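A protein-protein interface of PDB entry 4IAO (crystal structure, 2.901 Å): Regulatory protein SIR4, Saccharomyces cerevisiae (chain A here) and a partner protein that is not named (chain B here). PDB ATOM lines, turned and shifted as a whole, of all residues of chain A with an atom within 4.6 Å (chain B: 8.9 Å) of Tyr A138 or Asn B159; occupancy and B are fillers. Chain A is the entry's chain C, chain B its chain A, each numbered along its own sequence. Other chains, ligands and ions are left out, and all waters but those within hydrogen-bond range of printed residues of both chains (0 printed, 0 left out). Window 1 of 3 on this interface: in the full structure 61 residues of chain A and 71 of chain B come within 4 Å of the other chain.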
ATOM      1  N   GLY A 105      14.960   0.363   1.807  1.00  0.00           N
ATOM      2  CA  GLY A 105      13.569   0.193   2.184  1.00  0.00           C
ATOM      3  C   GLY A 105      12.913  -0.924   1.390  1.00  0.00           C
ATOM      4  O   GLY A 105      11.703  -1.130   1.452  1.00  0.00           O
ATOM      5  N   ILE A 106      13.724  -1.639   0.623  1.00  0.00           N
ATOM      6  CA  ILE A 106      13.247  -2.735  -0.204  1.00  0.00           C
ATOM      7  C   ILE A 106      13.839  -4.064   0.239  1.00  0.00           C
ATOM      8  O   ILE A 106      15.060  -4.216   0.273  1.00  0.00           O
ATOM      9  CB  ILE A 106      13.581  -2.505  -1.682  1.00  0.00           C
ATOM     10  CG1 ILE A 106      12.927  -1.216  -2.178  1.00  0.00           C
ATOM     11  CG2 ILE A 106      13.131  -3.689  -2.516  1.00  0.00           C
ATOM     12  CD1 ILE A 106      13.512  -0.724  -3.473  1.00  0.00           C
ATOM     13  N   PRO A 107      12.974  -5.028   0.591  1.00  0.00           N
ATOM     14  CA  PRO A 107      13.368  -6.376   1.025  1.00  0.00           C
ATOM     15  C   PRO A 107      14.250  -7.112   0.019  1.00  0.00           C
ATOM     16  O   PRO A 107      14.187  -6.824  -1.169  1.00  0.00           O
ATOM     17  CB  PRO A 107      12.024  -7.106   1.160  1.00  0.00           C
ATOM     18  CG  PRO A 107      11.027  -6.263   0.427  1.00  0.00           C
ATOM     19  CD  PRO A 107      11.510  -4.865   0.570  1.00  0.00           C
ATOM     20  N   SER A 134       6.187 -11.485   3.909  1.00  0.00           N
ATOM     21  CA  SER A 134       5.629 -10.154   4.084  1.00  0.00           C
ATOM     22  C   SER A 134       4.895  -9.727   2.817  1.00  0.00           C
ATOM     23  O   SER A 134       4.301  -8.651   2.760  1.00  0.00           O
ATOM     24  CB  SER A 134       6.743  -9.163   4.414  1.00  0.00           C
ATOM     25  OG  SER A 134       7.842  -9.322   3.530  1.00  0.00           O
ATOM     26  N   ALA A 135       4.943 -10.588   1.806  1.00  0.00           N
ATOM     27  CA  ALA A 135       4.388 -10.278   0.493  1.00  0.00           C
ATOM     28  C   ALA A 135       2.921  -9.873   0.559  1.00  0.00           C
ATOM     29  O   ALA A 135       2.495  -8.953  -0.134  1.00  0.00           O
ATOM     30  CB  ALA A 135       4.583 -11.448  -0.460  1.00  0.00           C
ATOM     31  N   PHE A 136       2.154 -10.557   1.401  1.00  0.00           N
ATOM     32  CA  PHE A 136       0.751 -10.216   1.603  1.00  0.00           C
ATOM     33  C   PHE A 136       0.593  -8.761   2.063  1.00  0.00           C
ATOM     34  O   PHE A 136      -0.410  -8.114   1.772  1.00  0.00           O
ATOM     35  CB  PHE A 136       0.110 -11.161   2.626  1.00  0.00           C
ATOM     36  CG  PHE A 136       0.487 -10.858   4.051  1.00  0.00           C
ATOM     37  CD1 PHE A 136      -0.343 -10.085   4.856  1.00  0.00           C
ATOM     38  CD2 PHE A 136       1.677 -11.329   4.583  1.00  0.00           C
ATOM     39  CE1 PHE A 136       0.003  -9.792   6.170  1.00  0.00           C
ATOM     40  CE2 PHE A 136       2.027 -11.038   5.895  1.00  0.00           C
ATOM     41  CZ  PHE A 136       1.189 -10.268   6.689  1.00  0.00           C
ATOM     42  N   PHE A 137       1.585  -8.249   2.786  1.00  0.00           N
ATOM     43  CA  PHE A 137       1.488  -6.915   3.363  1.00  0.00           C
ATOM     44  C   PHE A 137       1.776  -5.826   2.345  1.00  0.00           C
ATOM     45  O   PHE A 137       1.104  -4.794   2.320  1.00  0.00           O
ATOM     46  CB  PHE A 137       2.433  -6.772   4.556  1.00  0.00           C
ATOM     47  CG  PHE A 137       2.596  -5.353   5.035  1.00  0.00           C
ATOM     48  CD1 PHE A 137       1.535  -4.677   5.624  1.00  0.00           C
ATOM     49  CD2 PHE A 137       3.812  -4.697   4.901  1.00  0.00           C
ATOM     50  CE1 PHE A 137       1.681  -3.369   6.071  1.00  0.00           C
ATOM     51  CE2 PHE A 137       3.962  -3.387   5.346  1.00  0.00           C
ATOM     52  CZ  PHE A 137       2.897  -2.725   5.931  1.00  0.00           C
ATOM     53  N   TYR A 138       2.788  -6.055   1.517  1.00  0.00           N
ATOM     54  CA  TYR A 138       3.185  -5.081   0.510  1.00  0.00           C
ATOM     55  C   TYR A 138       2.177  -5.015  -0.633  1.00  0.00           C
ATOM     56  O   TYR A 138       1.883  -3.934  -1.145  1.00  0.00           O
ATOM     57  CB  TYR A 138       4.563  -5.427  -0.048  1.00  0.00           C
ATOM     58  CG  TYR A 138       5.701  -5.202   0.912  1.00  0.00           C
ATOM     59  CD1 TYR A 138       5.761  -4.061   1.694  1.00  0.00           C
ATOM     60  CD2 TYR A 138       6.718  -6.135   1.036  1.00  0.00           C
ATOM     61  CE1 TYR A 138       6.806  -3.851   2.573  1.00  0.00           C
ATOM     62  CE2 TYR A 138       7.767  -5.938   1.908  1.00  0.00           C
ATOM     63  CZ  TYR A 138       7.809  -4.793   2.676  1.00  0.00           C
ATOM     64  OH  TYR A 138       8.859  -4.596   3.549  1.00  0.00           O
ATOM     65  N   GLN A 139       1.646  -6.171  -1.025  1.00  0.00           N
ATOM     66  CA  GLN A 139       0.766  -6.237  -2.185  1.00  0.00           C
ATOM     67  C   GLN A 139      -0.624  -5.709  -1.865  1.00  0.00           C
ATOM     68  O   GLN A 139      -1.448  -5.510  -2.759  1.00  0.00           O
ATOM     69  CB  GLN A 139       0.713  -7.656  -2.783  1.00  0.00           C
ATOM     70  CG  GLN A 139      -0.061  -8.691  -1.981  1.00  0.00           C
ATOM     71  CD  GLN A 139       0.150 -10.107  -2.513  1.00  0.00           C
ATOM     72  OE1 GLN A 139       1.021 -10.345  -3.353  1.00  0.00           O
ATOM     73  NE2 GLN A 139      -0.646 -11.052  -2.024  1.00  0.00           N
ATOM     74  N   GLN A 140      -0.878  -5.462  -0.587  1.00  0.00           N
ATOM     75  CA  GLN A 140      -2.124  -4.828  -0.196  1.00  0.00           C
ATOM     76  C   GLN A 140      -1.873  -3.355   0.104  1.00  0.00           C
ATOM     77  O   GLN A 140      -1.259  -3.008   1.114  1.00  0.00           O
ATOM     78  CB  GLN A 140      -2.717  -5.522   1.033  1.00  0.00           C
ATOM     79  CG  GLN A 140      -3.274  -6.920   0.774  1.00  0.00           C
ATOM     80  CD  GLN A 140      -3.467  -7.720   2.059  1.00  0.00           C
ATOM     81  OE1 GLN A 140      -2.814  -7.456   3.070  1.00  0.00           O
ATOM     82  NE2 GLN A 140      -4.366  -8.703   2.023  1.00  0.00           N
ATOM     83  N   VAL A 141      -2.337  -2.490  -0.791  1.00  0.00           N
ATOM     84  CA  VAL A 141      -2.392  -1.065  -0.496  1.00  0.00           C
ATOM     85  C   VAL A 141      -3.842  -0.606  -0.619  1.00  0.00           C
ATOM     86  O   VAL A 141      -4.397  -0.514  -1.717  1.00  0.00           O
ATOM     87  CB  VAL A 141      -1.454  -0.243  -1.415  1.00  0.00           C
ATOM     88  CG1 VAL A 141      -1.492  -0.770  -2.846  1.00  0.00           C
ATOM     89  CG2 VAL A 141      -1.801   1.242  -1.357  1.00  0.00           C
ATOM     90  N   LEU B  72      11.387  -3.860 -13.647  1.00  0.00           N
ATOM     91  CA  LEU B  72      11.650  -3.978 -12.223  1.00  0.00           C
ATOM     92  C   LEU B  72      11.717  -5.441 -11.832  1.00  0.00           C
ATOM     93  O   LEU B  72      12.716  -5.905 -11.278  1.00  0.00           O
ATOM     94  CB  LEU B  72      10.553  -3.265 -11.429  1.00  0.00           C
ATOM     95  CG  LEU B  72      10.652  -3.282  -9.903  1.00  0.00           C
ATOM     96  CD1 LEU B  72      12.068  -2.967  -9.439  1.00  0.00           C
ATOM     97  CD2 LEU B  72       9.656  -2.293  -9.314  1.00  0.00           C
ATOM     98  N   LYS B  73      10.655  -6.170 -12.154  1.00  0.00           N
ATOM     99  CA  LYS B  73      10.552  -7.573 -11.788  1.00  0.00           C
ATOM    100  C   LYS B  73      11.536  -8.465 -12.553  1.00  0.00           C
ATOM    101  O   LYS B  73      11.905  -9.550 -12.089  1.00  0.00           O
ATOM    102  CB  LYS B  73       9.114  -8.055 -11.978  1.00  0.00           C
ATOM    103  CG  LYS B  73       8.088  -7.247 -11.197  1.00  0.00           C
ATOM    104  CD  LYS B  73       6.694  -7.834 -11.328  1.00  0.00           C
ATOM    105  CE  LYS B  73       6.602  -9.229 -10.728  1.00  0.00           C
ATOM    106  NZ  LYS B  73       6.536  -9.197  -9.246  1.00  0.00           N
ATOM    107  N   ALA B  77      15.567  -4.540  -8.345  1.00  0.00           N
ATOM    108  CA  ALA B  77      15.347  -3.142  -8.014  1.00  0.00           C
ATOM    109  C   ALA B  77      16.581  -2.315  -8.335  1.00  0.00           C
ATOM    110  O   ALA B  77      16.474  -1.179  -8.803  1.00  0.00           O
ATOM    111  CB  ALA B  77      14.963  -2.993  -6.542  1.00  0.00           C
ATOM    112  N   LEU B 101       5.862   4.106 -12.582  1.00  0.00           N
ATOM    113  CA  LEU B 101       5.435   2.769 -12.177  1.00  0.00           C
ATOM    114  C   LEU B 101       3.915   2.696 -12.081  1.00  0.00           C
ATOM    115  O   LEU B 101       3.354   1.720 -11.583  1.00  0.00           O
ATOM    116  CB  LEU B 101       6.105   2.346 -10.866  1.00  0.00           C
ATOM    117  CG  LEU B 101       7.557   1.898 -11.054  1.00  0.00           C
ATOM    118  CD1 LEU B 101       8.290   1.783  -9.728  1.00  0.00           C
ATOM    119  CD2 LEU B 101       7.605   0.575 -11.801  1.00  0.00           C
ATOM    120  N   PHE B 103       1.738   4.923 -10.482  1.00  0.00           N
ATOM    121  CA  PHE B 103       1.152   5.335  -9.206  1.00  0.00           C
ATOM    122  C   PHE B 103       0.916   6.834  -9.170  1.00  0.00           C
ATOM    123  O   PHE B 103       1.671   7.603  -9.759  1.00  0.00           O
ATOM    124  CB  PHE B 103       2.055   4.960  -8.033  1.00  0.00           C
ATOM    125  CG  PHE B 103       2.056   3.502  -7.713  1.00  0.00           C
ATOM    126  CD1 PHE B 103       1.015   2.943  -6.991  1.00  0.00           C
ATOM    127  CD2 PHE B 103       3.100   2.687  -8.127  1.00  0.00           C
ATOM    128  CE1 PHE B 103       1.012   1.602  -6.690  1.00  0.00           C
ATOM    129  CE2 PHE B 103       3.106   1.344  -7.830  1.00  0.00           C
ATOM    130  CZ  PHE B 103       2.061   0.798  -7.110  1.00  0.00           C
ATOM    131  N   ILE B 151      10.586   9.574  -0.875  1.00  0.00           N
ATOM    132  CA  ILE B 151      11.399   8.355  -0.813  1.00  0.00           C
ATOM    133  C   ILE B 151      10.652   7.168  -0.191  1.00  0.00           C
ATOM    134  O   ILE B 151      10.763   6.030  -0.659  1.00  0.00           O
ATOM    135  CB  ILE B 151      12.694   8.602  -0.013  1.00  0.00           C
ATOM    136  CG1 ILE B 151      13.569   9.635  -0.724  1.00  0.00           C
ATOM    137  CG2 ILE B 151      13.457   7.304   0.204  1.00  0.00           C
ATOM    138  CD1 ILE B 151      14.776  10.070   0.081  1.00  0.00           C
ATOM    139  N   LYS B 152       9.889   7.444   0.862  1.00  0.00           N
ATOM    140  CA  LYS B 152       9.045   6.433   1.480  1.00  0.00           C
ATOM    141  C   LYS B 152       8.063   5.865   0.470  1.00  0.00           C
ATOM    142  O   LYS B 152       8.034   4.658   0.227  1.00  0.00           O
ATOM    143  CB  LYS B 152       8.264   7.031   2.644  1.00  0.00           C
ATOM    144  CG  LYS B 152       9.070   7.236   3.902  1.00  0.00           C
ATOM    145  CD  LYS B 152       8.158   7.641   5.046  1.00  0.00           C
ATOM    146  CE  LYS B 152       8.912   7.706   6.350  1.00  0.00           C
ATOM    147  NZ  LYS B 152       9.642   6.435   6.628  1.00  0.00           N
ATOM    148  N   ASP B 153       7.266   6.745  -0.122  1.00  0.00           N
ATOM    149  CA  ASP B 153       6.228   6.326  -1.055  1.00  0.00           C
ATOM    150  C   ASP B 153       6.770   5.608  -2.283  1.00  0.00           C
ATOM    151  O   ASP B 153       6.072   4.800  -2.882  1.00  0.00           O
ATOM    152  CB  ASP B 153       5.355   7.511  -1.462  1.00  0.00           C
ATOM    153  CG  ASP B 153       4.340   7.868  -0.394  1.00  0.00           C
ATOM    154  OD1 ASP B 153       4.021   6.980   0.425  1.00  0.00           O
ATOM    155  OD2 ASP B 153       3.865   9.026  -0.373  1.00  0.00           O
ATOM    156  N   LEU B 154       8.012   5.897  -2.654  1.00  0.00           N
ATOM    157  CA  LEU B 154       8.646   5.182  -3.753  1.00  0.00           C
ATOM    158  C   LEU B 154       8.940   3.747  -3.334  1.00  0.00           C
ATOM    159  O   LEU B 154       8.693   2.806  -4.088  1.00  0.00           O
ATOM    160  CB  LEU B 154       9.937   5.867  -4.183  1.00  0.00           C
ATOM    161  CG  LEU B 154      10.607   5.166  -5.362  1.00  0.00           C
ATOM    162  CD1 LEU B 154       9.680   5.196  -6.574  1.00  0.00           C
ATOM    163  CD2 LEU B 154      11.949   5.798  -5.686  1.00  0.00           C
ATOM    164  N   GLN B 155       9.470   3.594  -2.124  1.00  0.00           N
ATOM    165  CA  GLN B 155       9.753   2.275  -1.566  1.00  0.00           C
ATOM    166  C   GLN B 155       8.488   1.431  -1.453  1.00  0.00           C
ATOM    167  O   GLN B 155       8.514   0.244  -1.743  1.00  0.00           O
ATOM    168  CB  GLN B 155      10.441   2.401  -0.205  1.00  0.00           C
ATOM    169  CG  GLN B 155      11.878   2.891  -0.281  1.00  0.00           C
ATOM    170  CD  GLN B 155      12.408   3.333   1.067  1.00  0.00           C
ATOM    171  OE1 GLN B 155      11.643   3.742   1.938  1.00  0.00           O
ATOM    172  NE2 GLN B 155      13.719   3.251   1.247  1.00  0.00           N
ATOM    173  N   ARG B 156       7.384   2.045  -1.036  1.00  0.00           N
ATOM    174  CA  ARG B 156       6.101   1.348  -0.986  1.00  0.00           C
ATOM    175  C   ARG B 156       5.693   0.903  -2.385  1.00  0.00           C
ATOM    176  O   ARG B 156       5.277  -0.242  -2.597  1.00  0.00           O
ATOM    177  CB  ARG B 156       5.010   2.238  -0.386  1.00  0.00           C
ATOM    178  CG  ARG B 156       5.086   2.396   1.118  1.00  0.00           C
ATOM    179  CD  ARG B 156       3.974   3.303   1.636  1.00  0.00           C
ATOM    180  NE  ARG B 156       4.167   3.669   3.039  1.00  0.00           N
ATOM    181  CZ  ARG B 156       4.793   4.771   3.452  1.00  0.00           C
ATOM    182  NH1 ARG B 156       5.291   5.626   2.567  1.00  0.00           N
ATOM    183  NH2 ARG B 156       4.920   5.021   4.751  1.00  0.00           N
ATOM    184  N   ALA B 157       5.820   1.820  -3.338  1.00  0.00           N
ATOM    185  CA  ALA B 157       5.465   1.549  -4.723  1.00  0.00           C
ATOM    186  C   ALA B 157       6.284   0.389  -5.285  1.00  0.00           C
ATOM    187  O   ALA B 157       5.726  -0.574  -5.812  1.00  0.00           O
ATOM    188  CB  ALA B 157       5.654   2.794  -5.565  1.00  0.00           C
ATOM    189  N   ILE B 158       7.605   0.484  -5.166  1.00  0.00           N
ATOM    190  CA  ILE B 158       8.487  -0.585  -5.611  1.00  0.00           C
ATOM    191  C   ILE B 158       8.131  -1.921  -4.972  1.00  0.00           C
ATOM    192  O   ILE B 158       8.101  -2.950  -5.651  1.00  0.00           O
ATOM    193  CB  ILE B 158       9.953  -0.257  -5.316  1.00  0.00           C
ATOM    194  CG1 ILE B 158      10.356   1.008  -6.074  1.00  0.00           C
ATOM    195  CG2 ILE B 158      10.855  -1.438  -5.686  1.00  0.00           C
ATOM    196  CD1 ILE B 158      11.805   1.399  -5.903  1.00  0.00           C
ATOM    197  N   ASN B 159       7.847  -1.902  -3.673  1.00  0.00           N
ATOM    198  CA  ASN B 159       7.500  -3.122  -2.957  1.00  0.00           C
ATOM    199  C   ASN B 159       6.156  -3.703  -3.393  1.00  0.00           C
ATOM    200  O   ASN B 159       5.990  -4.919  -3.439  1.00  0.00           O
ATOM    201  CB  ASN B 159       7.527  -2.902  -1.442  1.00  0.00           C
ATOM    202  CG  ASN B 159       8.920  -2.568  -0.916  1.00  0.00           C
ATOM    203  OD1 ASN B 159       9.061  -1.908   0.112  1.00  0.00           O
ATOM    204  ND2 ASN B 159       9.953  -3.012  -1.628  1.00  0.00           N
ATOM    205  N   LYS B 160       5.202  -2.832  -3.715  1.00  0.00           N
ATOM    206  CA  LYS B 160       3.891  -3.276  -4.187  1.00  0.00           C
ATOM    207  C   LYS B 160       4.002  -3.979  -5.539  1.00  0.00           C
ATOM    208  O   LYS B 160       3.354  -4.995  -5.766  1.00  0.00           O
ATOM    209  CB  LYS B 160       2.906  -2.101  -4.251  1.00  0.00           C
ATOM    210  CG  LYS B 160       1.689  -2.309  -5.155  1.00  0.00           C
ATOM    211  CD  LYS B 160       0.818  -3.478  -4.728  1.00  0.00           C
ATOM    212  CE  LYS B 160      -0.362  -3.644  -5.670  1.00  0.00           C
ATOM    213  NZ  LYS B 160      -0.886  -5.046  -5.711  1.00  0.00           N
ATOM    214  N   VAL B 161       4.829  -3.445  -6.429  1.00  0.00           N
ATOM    215  CA  VAL B 161       5.053  -4.079  -7.723  1.00  0.00           C
ATOM    216  C   VAL B 161       5.862  -5.371  -7.598  1.00  0.00           C
ATOM    217  O   VAL B 161       5.472  -6.401  -8.142  1.00  0.00           O
ATOM    218  CB  VAL B 161       5.732  -3.117  -8.715  1.00  0.00           C
ATOM    219  CG1 VAL B 161       6.300  -3.877  -9.909  1.00  0.00           C
ATOM    220  CG2 VAL B 161       4.740  -2.064  -9.168  1.00  0.00           C
ATOM    221  N   LEU B 162       6.979  -5.314  -6.878  1.00  0.00           N
ATOM    222  CA  LEU B 162       7.799  -6.498  -6.634  1.00  0.00           C
ATOM    223  C   LEU B 162       6.992  -7.642  -6.003  1.00  0.00           C
ATOM    224  O   LEU B 162       7.266  -8.820  -6.245  1.00  0.00           O
ATOM    225  CB  LEU B 162       9.006  -6.149  -5.756  1.00  0.00           C
ATOM    226  CG  LEU B 162      10.294  -5.725  -6.467  1.00  0.00           C
ATOM    227  CD1 LEU B 162      11.344  -5.244  -5.481  1.00  0.00           C
ATOM    228  CD2 LEU B 162      10.846  -6.869  -7.287  1.00  0.00           C
ATOM    229  N   CYS B 163       5.995  -7.290  -5.198  1.00  0.00           N
ATOM    230  CA  CYS B 163       5.143  -8.284  -4.547  1.00  0.00           C
ATOM    231  C   CYS B 163       3.833  -8.586  -5.270  1.00  0.00           C
ATOM    232  O   CYS B 163       2.998  -9.320  -4.738  1.00  0.00           O
ATOM    233  CB  CYS B 163       4.841  -7.880  -3.105  1.00  0.00           C
ATOM    234  SG  CYS B 163       6.168  -8.266  -1.979  1.00  0.00           S
ATOM    235  N   THR B 164       3.638  -8.001  -6.454  1.00  0.00           N
ATOM    236  CA  THR B 164       2.414  -8.234  -7.224  1.00  0.00           C
ATOM    237  C   THR B 164       2.673  -9.025  -8.501  1.00  0.00           C
ATOM    238  O   THR B 164       3.580  -8.703  -9.276  1.00  0.00           O
ATOM    239  CB  THR B 164       1.688  -6.915  -7.581  1.00  0.00           C
ATOM    240  OG1 THR B 164       1.241  -6.272  -6.382  1.00  0.00           O
ATOM    241  CG2 THR B 164       0.481  -7.186  -8.465  1.00  0.00           C
ATOM    242  N   ARG B 165       1.865 -10.058  -8.715  1.00  0.00           N
ATOM    243  CA  ARG B 165       1.950 -10.875  -9.921  1.00  0.00           C
ATOM    244  C   ARG B 165       1.552 -10.106 -11.181  1.00  0.00           C
ATOM    245  O   ARG B 165       0.614  -9.308 -11.161  1.00  0.00           O
ATOM    246  CB  ARG B 165       1.054 -12.101  -9.772  1.00  0.00           C
ATOM    247  CG  ARG B 165       1.045 -13.016 -10.971  1.00  0.00           C
ATOM    248  CD  ARG B 165       0.389 -14.334 -10.641  1.00  0.00           C
ATOM    249  NE  ARG B 165       0.655 -15.319 -11.676  1.00  0.00           N
ATOM    250  CZ  ARG B 165      -0.068 -15.435 -12.780  1.00  0.00           C
ATOM    251  NH1 ARG B 165      -1.099 -14.624 -12.973  1.00  0.00           N
ATOM    252  NH2 ARG B 165       0.239 -16.358 -13.683  1.00  0.00           N
ATOM    253  N   ASN B 414       1.302 -17.031  -4.143  1.00  0.00           N
ATOM    254  CA  ASN B 414       2.407 -16.067  -4.188  1.00  0.00           C
ATOM    255  C   ASN B 414       3.810 -16.656  -4.339  1.00  0.00           C
ATOM    256  O   ASN B 414       4.755 -15.937  -4.654  1.00  0.00           O
ATOM    257  CB  ASN B 414       2.383 -15.185  -2.937  1.00  0.00           C
ATOM    258  CG  ASN B 414       1.247 -14.193  -2.949  1.00  0.00           C
ATOM    259  OD1 ASN B 414       0.722 -13.842  -4.009  1.00  0.00           O
ATOM    260  ND2 ASN B 414       0.865 -13.721  -1.768  1.00  0.00           N
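O of Leu B162 is in hydrogen-bond range of NZ of Lys B73 (3.1 Å). O of Thr B164 lies within hydrogen-bond range of NZ of Lys B73 (3.0 Å). The backbone carbonyl oxygen (O) of Gln B155 sits close to the side-chain amide oxygen (OD1) of Asn B159. The side-chain sulfur (SG) of Cys B163 sits close to the backbone carbonyl oxygen (O) of Asn B159, 3.7 Å away. The side-chain hydroxyl (OG1) of Thr B164 is in hydrogen-bond range of the side-chain amino group (NZ) of Lys B160.
The backbone NH of Gly A105 lies close to the side-chain amide nitrogen of Gln B155 (3.2 Å). The side-chain amide oxygen of Asn B159 sits close to the backbone carbonyl oxygen of Gly A105. The backbone carbonyl oxygen of Gln A139 lies within hydrogen-bond range of the side-chain amino group of Lys B160 (3.0 Å). The backbone carbonyl oxygen of Cys B163 sits close to the side-chain amide oxygen of Gln A139. The side-chain amide nitrogen of Asn B414 lies close to the side-chain amide nitrogen of Gln A139, at 3.1 Å.
Hydrophobic or aromatic side chains of chain A that line the printed part of chain B: Ile A106, Pro A107, Ala A135 and Tyr A138. Printed residues of chain B that touch a printed residue of chain A: Gln B155, Ile B158, Asn B159, Lys B160, Leu B162, Cys B163, Thr B164 and Asn B414.
Among the printed residues, merely in contact across the chains: Ile A106 with Ile B158, Ile A106 with Asn B159, Ile A106 with Leu B162, Pro A107 with Asn B159, Ala A135 with Cys B163, Tyr A138 with Asn B159, Tyr A138 with Lys B160, Tyr A138 with Cys B163 and Gln A139 with Thr B164.
Of the printed residues of chain A, Asn B159 touches Gly A105, Ile A106, Pro A107 and Tyr A138. Printed residues of chain A within 4 Å of Ile B158: Ile A106 (3.5 Å). Of the printed residues of chain A, Leu B162 touches Ile A106 (3.8 Å). Printed residues of chain B within 4 Å of Pro A107: Asn B159. Of the printed residues of chain B, Gly A105 touches Gln B155 and Asn B159. Of the printed residues of chain B, Ile A106 touches Ile B158, Asn B159 and Leu B162.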
